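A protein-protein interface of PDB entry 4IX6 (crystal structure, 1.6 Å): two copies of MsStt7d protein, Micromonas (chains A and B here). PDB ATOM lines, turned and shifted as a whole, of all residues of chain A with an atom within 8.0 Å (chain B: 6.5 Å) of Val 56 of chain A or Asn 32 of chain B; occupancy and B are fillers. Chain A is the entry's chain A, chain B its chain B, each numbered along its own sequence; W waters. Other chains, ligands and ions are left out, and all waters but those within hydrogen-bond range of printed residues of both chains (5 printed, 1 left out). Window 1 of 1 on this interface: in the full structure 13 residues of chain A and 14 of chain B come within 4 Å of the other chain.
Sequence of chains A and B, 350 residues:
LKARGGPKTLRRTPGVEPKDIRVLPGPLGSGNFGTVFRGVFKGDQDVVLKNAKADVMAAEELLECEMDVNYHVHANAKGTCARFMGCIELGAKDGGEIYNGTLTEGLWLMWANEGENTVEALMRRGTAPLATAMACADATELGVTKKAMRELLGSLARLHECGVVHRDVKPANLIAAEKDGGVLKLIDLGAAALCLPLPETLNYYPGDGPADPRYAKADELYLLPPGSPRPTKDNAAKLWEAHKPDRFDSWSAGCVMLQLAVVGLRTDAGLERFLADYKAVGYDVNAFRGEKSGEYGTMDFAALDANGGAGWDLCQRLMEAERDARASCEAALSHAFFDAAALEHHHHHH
The side-chain hydroxyl of Ser 30 of chain B lies within hydrogen-bond range of the side-chain hydroxyl of Ser 30 of chain A.
NZ of Lys 53 of chain B is in hydrogen-bond range of O of Gly 31 of chain B (2.7 Å).
O of Phe 33 of chain B sits at hydrogen-bond distance from N of Lys 53 of chain B, at 2.7 Å.
The side-chain carboxylate (OD2) of Asp 212 of chain B lies within salt-bridge range of the guanidinium group (NH2) of Arg 214 of chain B, at 2.7 Å.
Among the printed residues, pairs that only touch across the chains: Ser 30 of chain A with Lys 53 of chain B, Asn 32 of chain A with Val 56 of chain B, Ala 54 of chain A with Asp 212 of chain B, Ala 54 of chain A with Pro 213 of chain B, Ala 54 of chain A with Arg 214 of chain B, Asp 55 of chain A with Ala 211 of chain B, Asp 55 of chain A with Asp 212 of chain B, Asp 55 of chain A with Pro 213 of chain B, Asp 55 of chain A with Arg 214 of chain B, Val 56 of chain A with Asn 32 of chain B, Val 56 of chain A with Pro 213 of chain B, Met 57 of chain A with Ala 211 of chain B and Met 57 of chain A with Pro 213 of chain B.
Val 56 of chain A touches just these residues of chain B: Asn 32 and Pro 213.
No residue of chain A comes within 4 Å of Gly 31 of chain B.
Of chain A, only Val 56 (3.7 Å) comes within 4 Å of Asn 32 of chain B.
Printed residues of chain A within 4 Å of Val 56 of chain B: Asn 32.
Ala 59 of chain B touches none of the printed residues of chain A.
Of the printed residues of chain A, Pro 213 of chain B touches Ala 54 (3.8 Å), Asp 55 (3.7 Å), Val 56 (3.8 Å) and Met 57 (3.8 Å).
Printed residues of chain A within 4 Å of Arg 214 of chain B: Ala 54 (3.5 Å) and Asp 55 (3.7 Å).
The nearest residue of chain A that does not touch Asn 32 of chain B is Asn 32 of chain A (4.3 Å).
Hydrophobic or aromatic side chains of chain A that line the printed part of chain B: Val 56 and Met 57.
Hydrophobic or aromatic side chains of chain B within 4 Å of the printed part of chain A: Val 56, Ala 211 and Pro 213.
Among the printed residues, 14 pairs touch across the chains.
Ser 30 of chain B touches its own counterpart, Ser 30 of chain A.
Ser 30 of chain A touches Lys 53 of chain B, but with the chains exchanged Lys 53 of chain A does not touch Ser 30 of chain B (4.4 Å).
Asn 32 of chain A touches Val 56 of chain B, and with the chains exchanged Val 56 of chain A touches Asn 32 of chain B.
Positions printed for both chains: 30, 31, 32, 33, 34, 53, 56, 59 and 62.
Water W4 lies within hydrogen-bond range of O of Asn 32 of chain A (2.6 Å) and ND2 of Asn 32 of chain B (3.0 Å).
Water W5 lies within hydrogen-bond range of OD1 of Asn 32 of chain A (2.7 Å) and O of Asn 32 of chain B (2.7 Å).
Water W3 bridges the backbone carbonyl oxygen of Asp 55 of chain A (2.7 Å) and the side-chain amide oxygen of Asn 32 of chain B (3.1 Å).
Water W2 bridges the backbone carbonyl oxygen (O) of Ser 30 of chain B and the side-chain carboxylate (OD2) of Asp 55 of chain A.
Water W1 lies within hydrogen-bond range of O of Ala 211 of chain B (3.0 Å) and N of Met 57 of chain A (3.0 Å).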
ATOM      1  N   SER A  30      -6.341   3.329  -4.134  1.00  0.00           N
ATOM      2  CA  SER A  30      -5.279   3.844  -3.289  1.00  0.00           C
ATOM      3  C   SER A  30      -4.695   2.688  -2.504  1.00  0.00           C
ATOM      4  O   SER A  30      -5.419   1.789  -2.068  1.00  0.00           O
ATOM      5  CB  SER A  30      -5.841   4.877  -2.317  1.00  0.00           C
ATOM      6  OG  SER A  30      -6.854   4.290  -1.521  1.00  0.00           O
ATOM      7  N   GLY A  31      -3.381   2.714  -2.326  1.00  0.00           N
ATOM      8  CA  GLY A  31      -2.705   1.687  -1.564  1.00  0.00           C
ATOM      9  C   GLY A  31      -2.197   2.268  -0.267  1.00  0.00           C
ATOM     10  O   GLY A  31      -2.621   3.347   0.154  1.00  0.00           O
ATOM     11  N   ASN A  32      -1.281   1.556   0.372  1.00  0.00           N
ATOM     12  CA  ASN A  32      -0.727   2.020   1.630  1.00  0.00           C
ATOM     13  C   ASN A  32      -0.121   3.419   1.532  1.00  0.00           C
ATOM     14  O   ASN A  32      -0.265   4.220   2.455  1.00  0.00           O
ATOM     15  CB  ASN A  32       0.291   1.013   2.178  1.00  0.00           C
ATOM     16  CG  ASN A  32      -0.326  -0.352   2.444  1.00  0.00           C
ATOM     17  OD1 ASN A  32      -1.216  -0.490   3.283  1.00  0.00           O
ATOM     18  ND2 ASN A  32       0.151  -1.369   1.735  1.00  0.00           N
ATOM     19  N   PHE A  33       0.535   3.726   0.414  1.00  0.00           N
ATOM     20  CA  PHE A  33       1.295   4.969   0.347  1.00  0.00           C
ATOM     21  C   PHE A  33       1.042   5.831  -0.895  1.00  0.00           C
ATOM     22  O   PHE A  33       1.589   6.924  -1.005  1.00  0.00           O
ATOM     23  CB  PHE A  33       2.796   4.693   0.509  1.00  0.00           C
ATOM     24  CG  PHE A  33       3.385   3.828  -0.587  1.00  0.00           C
ATOM     25  CD1 PHE A  33       3.818   4.390  -1.785  1.00  0.00           C
ATOM     26  CD2 PHE A  33       3.526   2.455  -0.404  1.00  0.00           C
ATOM     27  CE1 PHE A  33       4.370   3.605  -2.789  1.00  0.00           C
ATOM     28  CE2 PHE A  33       4.061   1.661  -1.403  1.00  0.00           C
ATOM     29  CZ  PHE A  33       4.493   2.240  -2.601  1.00  0.00           C
ATOM     30  N   GLY A  34       0.223   5.362  -1.829  1.00  0.00           N
ATOM     31  CA  GLY A  34       0.030   6.110  -3.060  1.00  0.00           C
ATOM     32  C   GLY A  34      -1.377   6.053  -3.615  1.00  0.00           C
ATOM     33  O   GLY A  34      -2.205   5.272  -3.154  1.00  0.00           O
ATOM     34  N   ALA A  52       2.517   9.783  -4.708  1.00  0.00           N
ATOM     35  CA  ALA A  52       2.619   9.458  -3.292  1.00  0.00           C
ATOM     36  C   ALA A  52       1.602  10.236  -2.463  1.00  0.00           C
ATOM     37  O   ALA A  52       1.362  11.422  -2.713  1.00  0.00           O
ATOM     38  CB  ALA A  52       4.035   9.729  -2.783  1.00  0.00           C
ATOM     39  N   LYS A  53       1.026   9.565  -1.468  1.00  0.00           N
ATOM     40  CA  LYS A  53       0.085  10.194  -0.552  1.00  0.00           C
ATOM     41  C   LYS A  53       0.765  11.219   0.328  1.00  0.00           C
ATOM     42  O   LYS A  53       1.812  10.953   0.922  1.00  0.00           O
ATOM     43  CB  LYS A  53      -0.593   9.138   0.317  1.00  0.00           C
ATOM     44  CG  LYS A  53      -1.665   8.359  -0.415  1.00  0.00           C
ATOM     45  CD  LYS A  53      -2.306   7.356   0.507  1.00  0.00           C
ATOM     46  CE  LYS A  53      -3.455   6.661  -0.180  1.00  0.00           C
ATOM     47  NZ  LYS A  53      -4.154   5.763   0.771  1.00  0.00           N
ATOM     48  N   ALA A  54       0.157  12.396   0.413  1.00  0.00           N
ATOM     49  CA  ALA A  54       0.721  13.485   1.197  1.00  0.00           C
ATOM     50  C   ALA A  54       0.599  13.238   2.699  1.00  0.00           C
ATOM     51  O   ALA A  54       1.322  13.841   3.499  1.00  0.00           O
ATOM     52  CB  ALA A  54       0.043  14.800   0.822  1.00  0.00           C
ATOM     53  N   ASP A  55      -0.312  12.350   3.076  1.00  0.00           N
ATOM     54  CA  ASP A  55      -0.639  12.144   4.480  1.00  0.00           C
ATOM     55  C   ASP A  55      -0.034  10.873   5.059  1.00  0.00           C
ATOM     56  O   ASP A  55      -0.397  10.454   6.159  1.00  0.00           O
ATOM     57  CB  ASP A  55      -2.160  12.140   4.668  1.00  0.00           C
ATOM     58  CG  ASP A  55      -2.845  11.021   3.900  1.00  0.00           C
ATOM     59  OD1 ASP A  55      -2.414  10.706   2.773  1.00  0.00           O
ATOM     60  OD2 ASP A  55      -3.824  10.452   4.426  1.00  0.00           O
ATOM     61  N   VAL A  56       0.881  10.255   4.316  1.00  0.00           N
ATOM     62  CA  VAL A  56       1.484   8.995   4.738  1.00  0.00           C
ATOM     63  C   VAL A  56       2.987   9.119   4.921  1.00  0.00           C
ATOM     64  O   VAL A  56       3.708   9.615   4.040  1.00  0.00           O
ATOM     65  CB  VAL A  56       1.189   7.861   3.736  1.00  0.00           C
ATOM     66  CG1 VAL A  56       2.002   6.629   4.090  1.00  0.00           C
ATOM     67  CG2 VAL A  56      -0.309   7.539   3.710  1.00  0.00           C
ATOM     68  N   MET A  57       3.448   8.678   6.083  1.00  0.00           N
ATOM     69  CA  MET A  57       4.859   8.681   6.431  1.00  0.00           C
ATOM     70  C   MET A  57       5.707   7.956   5.375  1.00  0.00           C
ATOM     71  O   MET A  57       5.376   6.838   4.979  1.00  0.00           O
ATOM     72  CB  MET A  57       5.001   7.977   7.779  1.00  0.00           C
ATOM     73  CG  MET A  57       6.376   7.992   8.398  1.00  0.00           C
ATOM     74  SD  MET A  57       6.300   7.157  10.004  1.00  0.00           S
ATOM     75  CE  MET A  57       4.985   8.104  10.762  1.00  0.00           C
ATOM     76  N   ALA A  58       6.764   8.613   4.899  1.00  0.00           N
ATOM     77  CA  ALA A  58       7.734   8.012   3.972  1.00  0.00           C
ATOM     78  C   ALA A  58       7.180   7.662   2.593  1.00  0.00           C
ATOM     79  O   ALA A  58       7.774   6.851   1.871  1.00  0.00           O
ATOM     80  CB  ALA A  58       8.389   6.784   4.600  1.00  0.00           C
ATOM     81  N   ALA A  59       6.063   8.271   2.216  1.00  0.00           N
ATOM     82  CA  ALA A  59       5.370   7.874   0.995  1.00  0.00           C
ATOM     83  C   ALA A  59       6.234   8.057  -0.246  1.00  0.00           C
ATOM     84  O   ALA A  59       6.251   7.188  -1.115  1.00  0.00           O
ATOM     85  CB  ALA A  59       4.056   8.642   0.851  1.00  0.00           C
ATOM     86  N   GLU A  60       6.954   9.177  -0.320  1.00  0.00           N
ATOM     87  CA  GLU A  60       7.782   9.459  -1.490  1.00  0.00           C
ATOM     88  C   GLU A  60       8.897   8.429  -1.605  1.00  0.00           C
ATOM     89  O   GLU A  60       9.206   7.966  -2.695  1.00  0.00           O
ATOM     90  CB  GLU A  60       8.372  10.873  -1.426  1.00  0.00           C
ATOM     91  CG  GLU A  60       7.446  11.963  -1.963  1.00  0.00           C
ATOM     92  CD  GLU A  60       7.899  12.513  -3.310  1.00  0.00           C
ATOM     93  OE1 GLU A  60       7.119  12.429  -4.288  1.00  0.00           O
ATOM     94  OE2 GLU A  60       9.035  13.039  -3.387  1.00  0.00           O
ATOM     95  N   GLU A  61       9.493   8.075  -0.472  1.00  0.00           N
ATOM     96  CA  GLU A  61      10.565   7.088  -0.447  1.00  0.00           C
ATOM     97  C   GLU A  61      10.050   5.703  -0.850  1.00  0.00           C
ATOM     98  O   GLU A  61      10.740   4.954  -1.552  1.00  0.00           O
ATOM     99  CB  GLU A  61      11.216   7.036   0.938  1.00  0.00           C
ATOM    100  CG  GLU A  61      12.140   8.222   1.251  1.00  0.00           C
ATOM    101  CD  GLU A  61      11.396   9.514   1.570  1.00  0.00           C
ATOM    102  OE1 GLU A  61      10.261   9.447   2.093  1.00  0.00           O
ATOM    103  OE2 GLU A  61      11.955  10.601   1.297  1.00  0.00           O
ATOM    104  N   LEU A  62       8.842   5.366  -0.408  1.00  0.00           N
ATOM    105  CA  LEU A  62       8.222   4.097  -0.793  1.00  0.00           C
ATOM    106  C   LEU A  62       7.974   4.071  -2.293  1.00  0.00           C
ATOM    107  O   LEU A  62       8.242   3.057  -2.962  1.00  0.00           O
ATOM    108  CB  LEU A  62       6.913   3.872  -0.019  1.00  0.00           C
ATOM    109  CG  LEU A  62       7.164   3.593   1.463  1.00  0.00           C
ATOM    110  CD1 LEU A  62       5.914   3.831   2.302  1.00  0.00           C
ATOM    111  CD2 LEU A  62       7.692   2.169   1.639  1.00  0.00           C
ATOM    112  N   SER B  30     -10.647   7.149   1.974  1.00  0.00           N
ATOM    113  CA  SER B  30     -10.066   5.939   2.525  1.00  0.00           C
ATOM    114  C   SER B  30      -8.741   6.304   3.151  1.00  0.00           C
ATOM    115  O   SER B  30      -7.943   7.039   2.566  1.00  0.00           O
ATOM    116  CB  SER B  30      -9.874   4.870   1.449  1.00  0.00           C
ATOM    117  OG  SER B  30      -8.689   5.105   0.712  1.00  0.00           O
ATOM    118  N   GLY B  31      -8.525   5.798   4.356  1.00  0.00           N
ATOM    119  CA  GLY B  31      -7.337   6.127   5.102  1.00  0.00           C
ATOM    120  C   GLY B  31      -6.372   4.979   5.022  1.00  0.00           C
ATOM    121  O   GLY B  31      -6.296   4.291   4.005  1.00  0.00           O
ATOM    122  N   ASN B  32      -5.626   4.771   6.097  1.00  0.00           N
ATOM    123  CA  ASN B  32      -4.615   3.734   6.105  1.00  0.00           C
ATOM    124  C   ASN B  32      -5.205   2.332   6.136  1.00  0.00           C
ATOM    125  O   ASN B  32      -4.668   1.419   5.513  1.00  0.00           O
ATOM    126  CB  ASN B  32      -3.645   3.933   7.269  1.00  0.00           C
ATOM    127  CG  ASN B  32      -2.792   5.175   7.103  1.00  0.00           C
ATOM    128  OD1 ASN B  32      -2.371   5.794   8.080  1.00  0.00           O
ATOM    129  ND2 ASN B  32      -2.544   5.553   5.853  1.00  0.00           N
ATOM    130  N   PHE B  33      -6.311   2.153   6.848  1.00  0.00           N
ATOM    131  CA  PHE B  33      -6.778   0.799   7.095  1.00  0.00           C
ATOM    132  C   PHE B  33      -8.262   0.602   6.863  1.00  0.00           C
ATOM    133  O   PHE B  33      -8.768  -0.502   7.046  1.00  0.00           O
ATOM    134  CB  PHE B  33      -6.399   0.334   8.506  1.00  0.00           C
ATOM    135  CG  PHE B  33      -7.111   1.085   9.610  1.00  0.00           C
ATOM    136  CD1 PHE B  33      -8.378   0.707  10.025  1.00  0.00           C
ATOM    137  CD2 PHE B  33      -6.494   2.165  10.238  1.00  0.00           C
ATOM    138  CE1 PHE B  33      -9.042   1.401  11.049  1.00  0.00           C
ATOM    139  CE2 PHE B  33      -7.143   2.858  11.259  1.00  0.00           C
ATOM    140  CZ  PHE B  33      -8.424   2.469  11.664  1.00  0.00           C
ATOM    141  N   GLY B  34      -8.951   1.660   6.457  1.00  0.00           N
ATOM    142  CA  GLY B  34     -10.394   1.576   6.262  1.00  0.00           C
ATOM    143  C   GLY B  34     -10.940   2.432   5.135  1.00  0.00           C
ATOM    144  O   GLY B  34     -10.218   3.228   4.521  1.00  0.00           O
ATOM    145  N   LYS B  50     -17.949   3.270   8.114  1.00  0.00           N
ATOM    146  CA  LYS B  50     -16.560   2.848   7.861  1.00  0.00           C
ATOM    147  C   LYS B  50     -16.399   1.343   8.014  1.00  0.00           C
ATOM    148  O   LYS B  50     -16.873   0.761   8.994  1.00  0.00           O
ATOM    149  CB  LYS B  50     -15.587   3.548   8.826  1.00  0.00           C
ATOM    150  CG  LYS B  50     -14.099   3.226   8.555  1.00  0.00           C
ATOM    151  CD  LYS B  50     -13.176   4.002   9.503  1.00  0.00           C
ATOM    152  CE  LYS B  50     -11.718   3.730   9.152  1.00  0.00           C
ATOM    153  NZ  LYS B  50     -10.734   4.489   9.967  1.00  0.00           N
ATOM    154  N   LYS B  53     -10.219  -2.131   5.383  1.00  0.00           N
ATOM    155  CA  LYS B  53      -9.674  -2.584   4.105  1.00  0.00           C
ATOM    156  C   LYS B  53      -9.260  -4.050   4.192  1.00  0.00           C
ATOM    157  O   LYS B  53      -8.539  -4.451   5.105  1.00  0.00           O
ATOM    158  CB  LYS B  53      -8.478  -1.730   3.722  1.00  0.00           C
ATOM    159  CG  LYS B  53      -8.876  -0.367   3.190  1.00  0.00           C
ATOM    160  CD  LYS B  53      -7.639   0.445   2.931  1.00  0.00           C
ATOM    161  CE  LYS B  53      -7.976   1.759   2.273  1.00  0.00           C
ATOM    162  NZ  LYS B  53      -6.722   2.510   1.998  1.00  0.00           N
ATOM    163  N   VAL B  56      -5.223  -4.864   4.051  1.00  0.00           N
ATOM    164  CA  VAL B  56      -4.282  -4.296   5.005  1.00  0.00           C
ATOM    165  C   VAL B  56      -4.155  -5.152   6.256  1.00  0.00           C
ATOM    166  O   VAL B  56      -5.151  -5.509   6.887  1.00  0.00           O
ATOM    167  CB  VAL B  56      -4.705  -2.877   5.421  1.00  0.00           C
ATOM    168  CG1 VAL B  56      -3.722  -2.318   6.430  1.00  0.00           C
ATOM    169  CG2 VAL B  56      -4.799  -1.986   4.196  1.00  0.00           C
ATOM    170  N   ALA B  59      -6.041  -4.588   9.771  1.00  0.00           N
ATOM    171  CA  ALA B  59      -7.007  -3.502   9.642  1.00  0.00           C
ATOM    172  C   ALA B  59      -8.183  -3.822  10.545  1.00  0.00           C
ATOM    173  O   ALA B  59      -8.807  -2.939  11.129  1.00  0.00           O
ATOM    174  CB  ALA B  59      -7.465  -3.367   8.204  1.00  0.00           C
ATOM    175  N   LEU B  62      -7.255  -2.692  13.926  1.00  0.00           N
ATOM    176  CA  LEU B  62      -7.254  -1.229  13.991  1.00  0.00           C
ATOM    177  C   LEU B  62      -8.664  -0.663  14.048  1.00  0.00           C
ATOM    178  O   LEU B  62      -8.922   0.305  14.771  1.00  0.00           O
ATOM    179  CB  LEU B  62      -6.493  -0.637  12.814  1.00  0.00           C
ATOM    180  CG  LEU B  62      -5.002  -0.927  12.910  1.00  0.00           C
ATOM    181  CD1 LEU B  62      -4.355  -0.768  11.548  1.00  0.00           C
ATOM    182  CD2 LEU B  62      -4.356  -0.016  13.948  1.00  0.00           C
ATOM    183  N   PRO B 210       1.512   5.509  13.020  1.00  0.00           N
ATOM    184  CA  PRO B 210       1.136   6.263  11.827  1.00  0.00           C
ATOM    185  C   PRO B 210       1.219   7.741  12.150  1.00  0.00           C
ATOM    186  O   PRO B 210       0.967   8.156  13.282  1.00  0.00           O
ATOM    187  CB  PRO B 210      -0.318   5.848  11.598  1.00  0.00           C
ATOM    188  CG  PRO B 210      -0.824   5.526  12.965  1.00  0.00           C
ATOM    189  CD  PRO B 210       0.345   4.910  13.691  1.00  0.00           C
ATOM    190  N   ALA B 211       1.607   8.534  11.171  1.00  0.00           N
ATOM    191  CA  ALA B 211       1.606   9.963  11.359  1.00  0.00           C
ATOM    192  C   ALA B 211       1.506  10.616  10.002  1.00  0.00           C
ATOM    193  O   ALA B 211       2.102  10.150   9.023  1.00  0.00           O
ATOM    194  CB  ALA B 211       2.874  10.408  12.081  1.00  0.00           C
ATOM    195  N   ASP B 212       0.733  11.690   9.946  1.00  0.00           N
ATOM    196  CA  ASP B 212       0.691  12.522   8.771  1.00  0.00           C
ATOM    197  C   ASP B 212       1.917  13.418   8.892  1.00  0.00           C
ATOM    198  O   ASP B 212       2.014  14.216   9.822  1.00  0.00           O
ATOM    199  CB  ASP B 212      -0.607  13.335   8.765  1.00  0.00           C
ATOM    200  CG  ASP B 212      -0.786  14.134   7.501  1.00  0.00           C
ATOM    201  OD1 ASP B 212       0.236  14.589   6.938  1.00  0.00           O
ATOM    202  OD2 ASP B 212      -1.944  14.310   7.075  1.00  0.00           O
ATOM    203  N   PRO B 213       2.891  13.256   7.985  1.00  0.00           N
ATOM    204  CA  PRO B 213       4.129  14.023   8.150  1.00  0.00           C
ATOM    205  C   PRO B 213       3.919  15.536   8.109  1.00  0.00           C
ATOM    206  O   PRO B 213       4.745  16.279   8.641  1.00  0.00           O
ATOM    207  CB  PRO B 213       5.002  13.552   6.977  1.00  0.00           C
ATOM    208  CG  PRO B 213       4.072  12.931   6.004  1.00  0.00           C
ATOM    209  CD  PRO B 213       2.894  12.407   6.782  1.00  0.00           C
ATOM    210  N   ARG B 214       2.826  15.987   7.498  1.00  0.00           N
ATOM    211  CA  ARG B 214       2.581  17.421   7.378  1.00  0.00           C
ATOM    212  C   ARG B 214       2.268  18.044   8.731  1.00  0.00           C
ATOM    213  O   ARG B 214       2.524  19.238   8.949  1.00  0.00           O
ATOM    214  CB  ARG B 214       1.418  17.700   6.416  1.00  0.00           C
ATOM    215  CG  ARG B 214       1.647  17.170   5.001  1.00  0.00           C
ATOM    216  CD  ARG B 214       0.385  17.262   4.168  1.00  0.00           C
ATOM    217  NE  ARG B 214      -0.690  16.451   4.733  1.00  0.00           N
ATOM    218  CZ  ARG B 214      -1.961  16.518   4.357  1.00  0.00           C
ATOM    219  NH1 ARG B 214      -2.337  17.357   3.399  1.00  0.00           N
ATOM    220  NH2 ARG B 214      -2.863  15.742   4.950  1.00  0.00           N
HETATM  221  O   HOH W   1       1.669   7.333   8.130  1.00  0.00           O
HETATM  222  O   HOH W   2      -6.453   9.349   2.829  1.00  0.00           O
HETATM  223  O   HOH W   3      -1.046   8.594   8.019  1.00  0.00           O
HETATM  224  O   HOH W   4      -0.605   3.495   4.928  1.00  0.00           O
HETATM  225  O   HOH W   5      -1.957   1.231   5.224  1.00  0.00           O
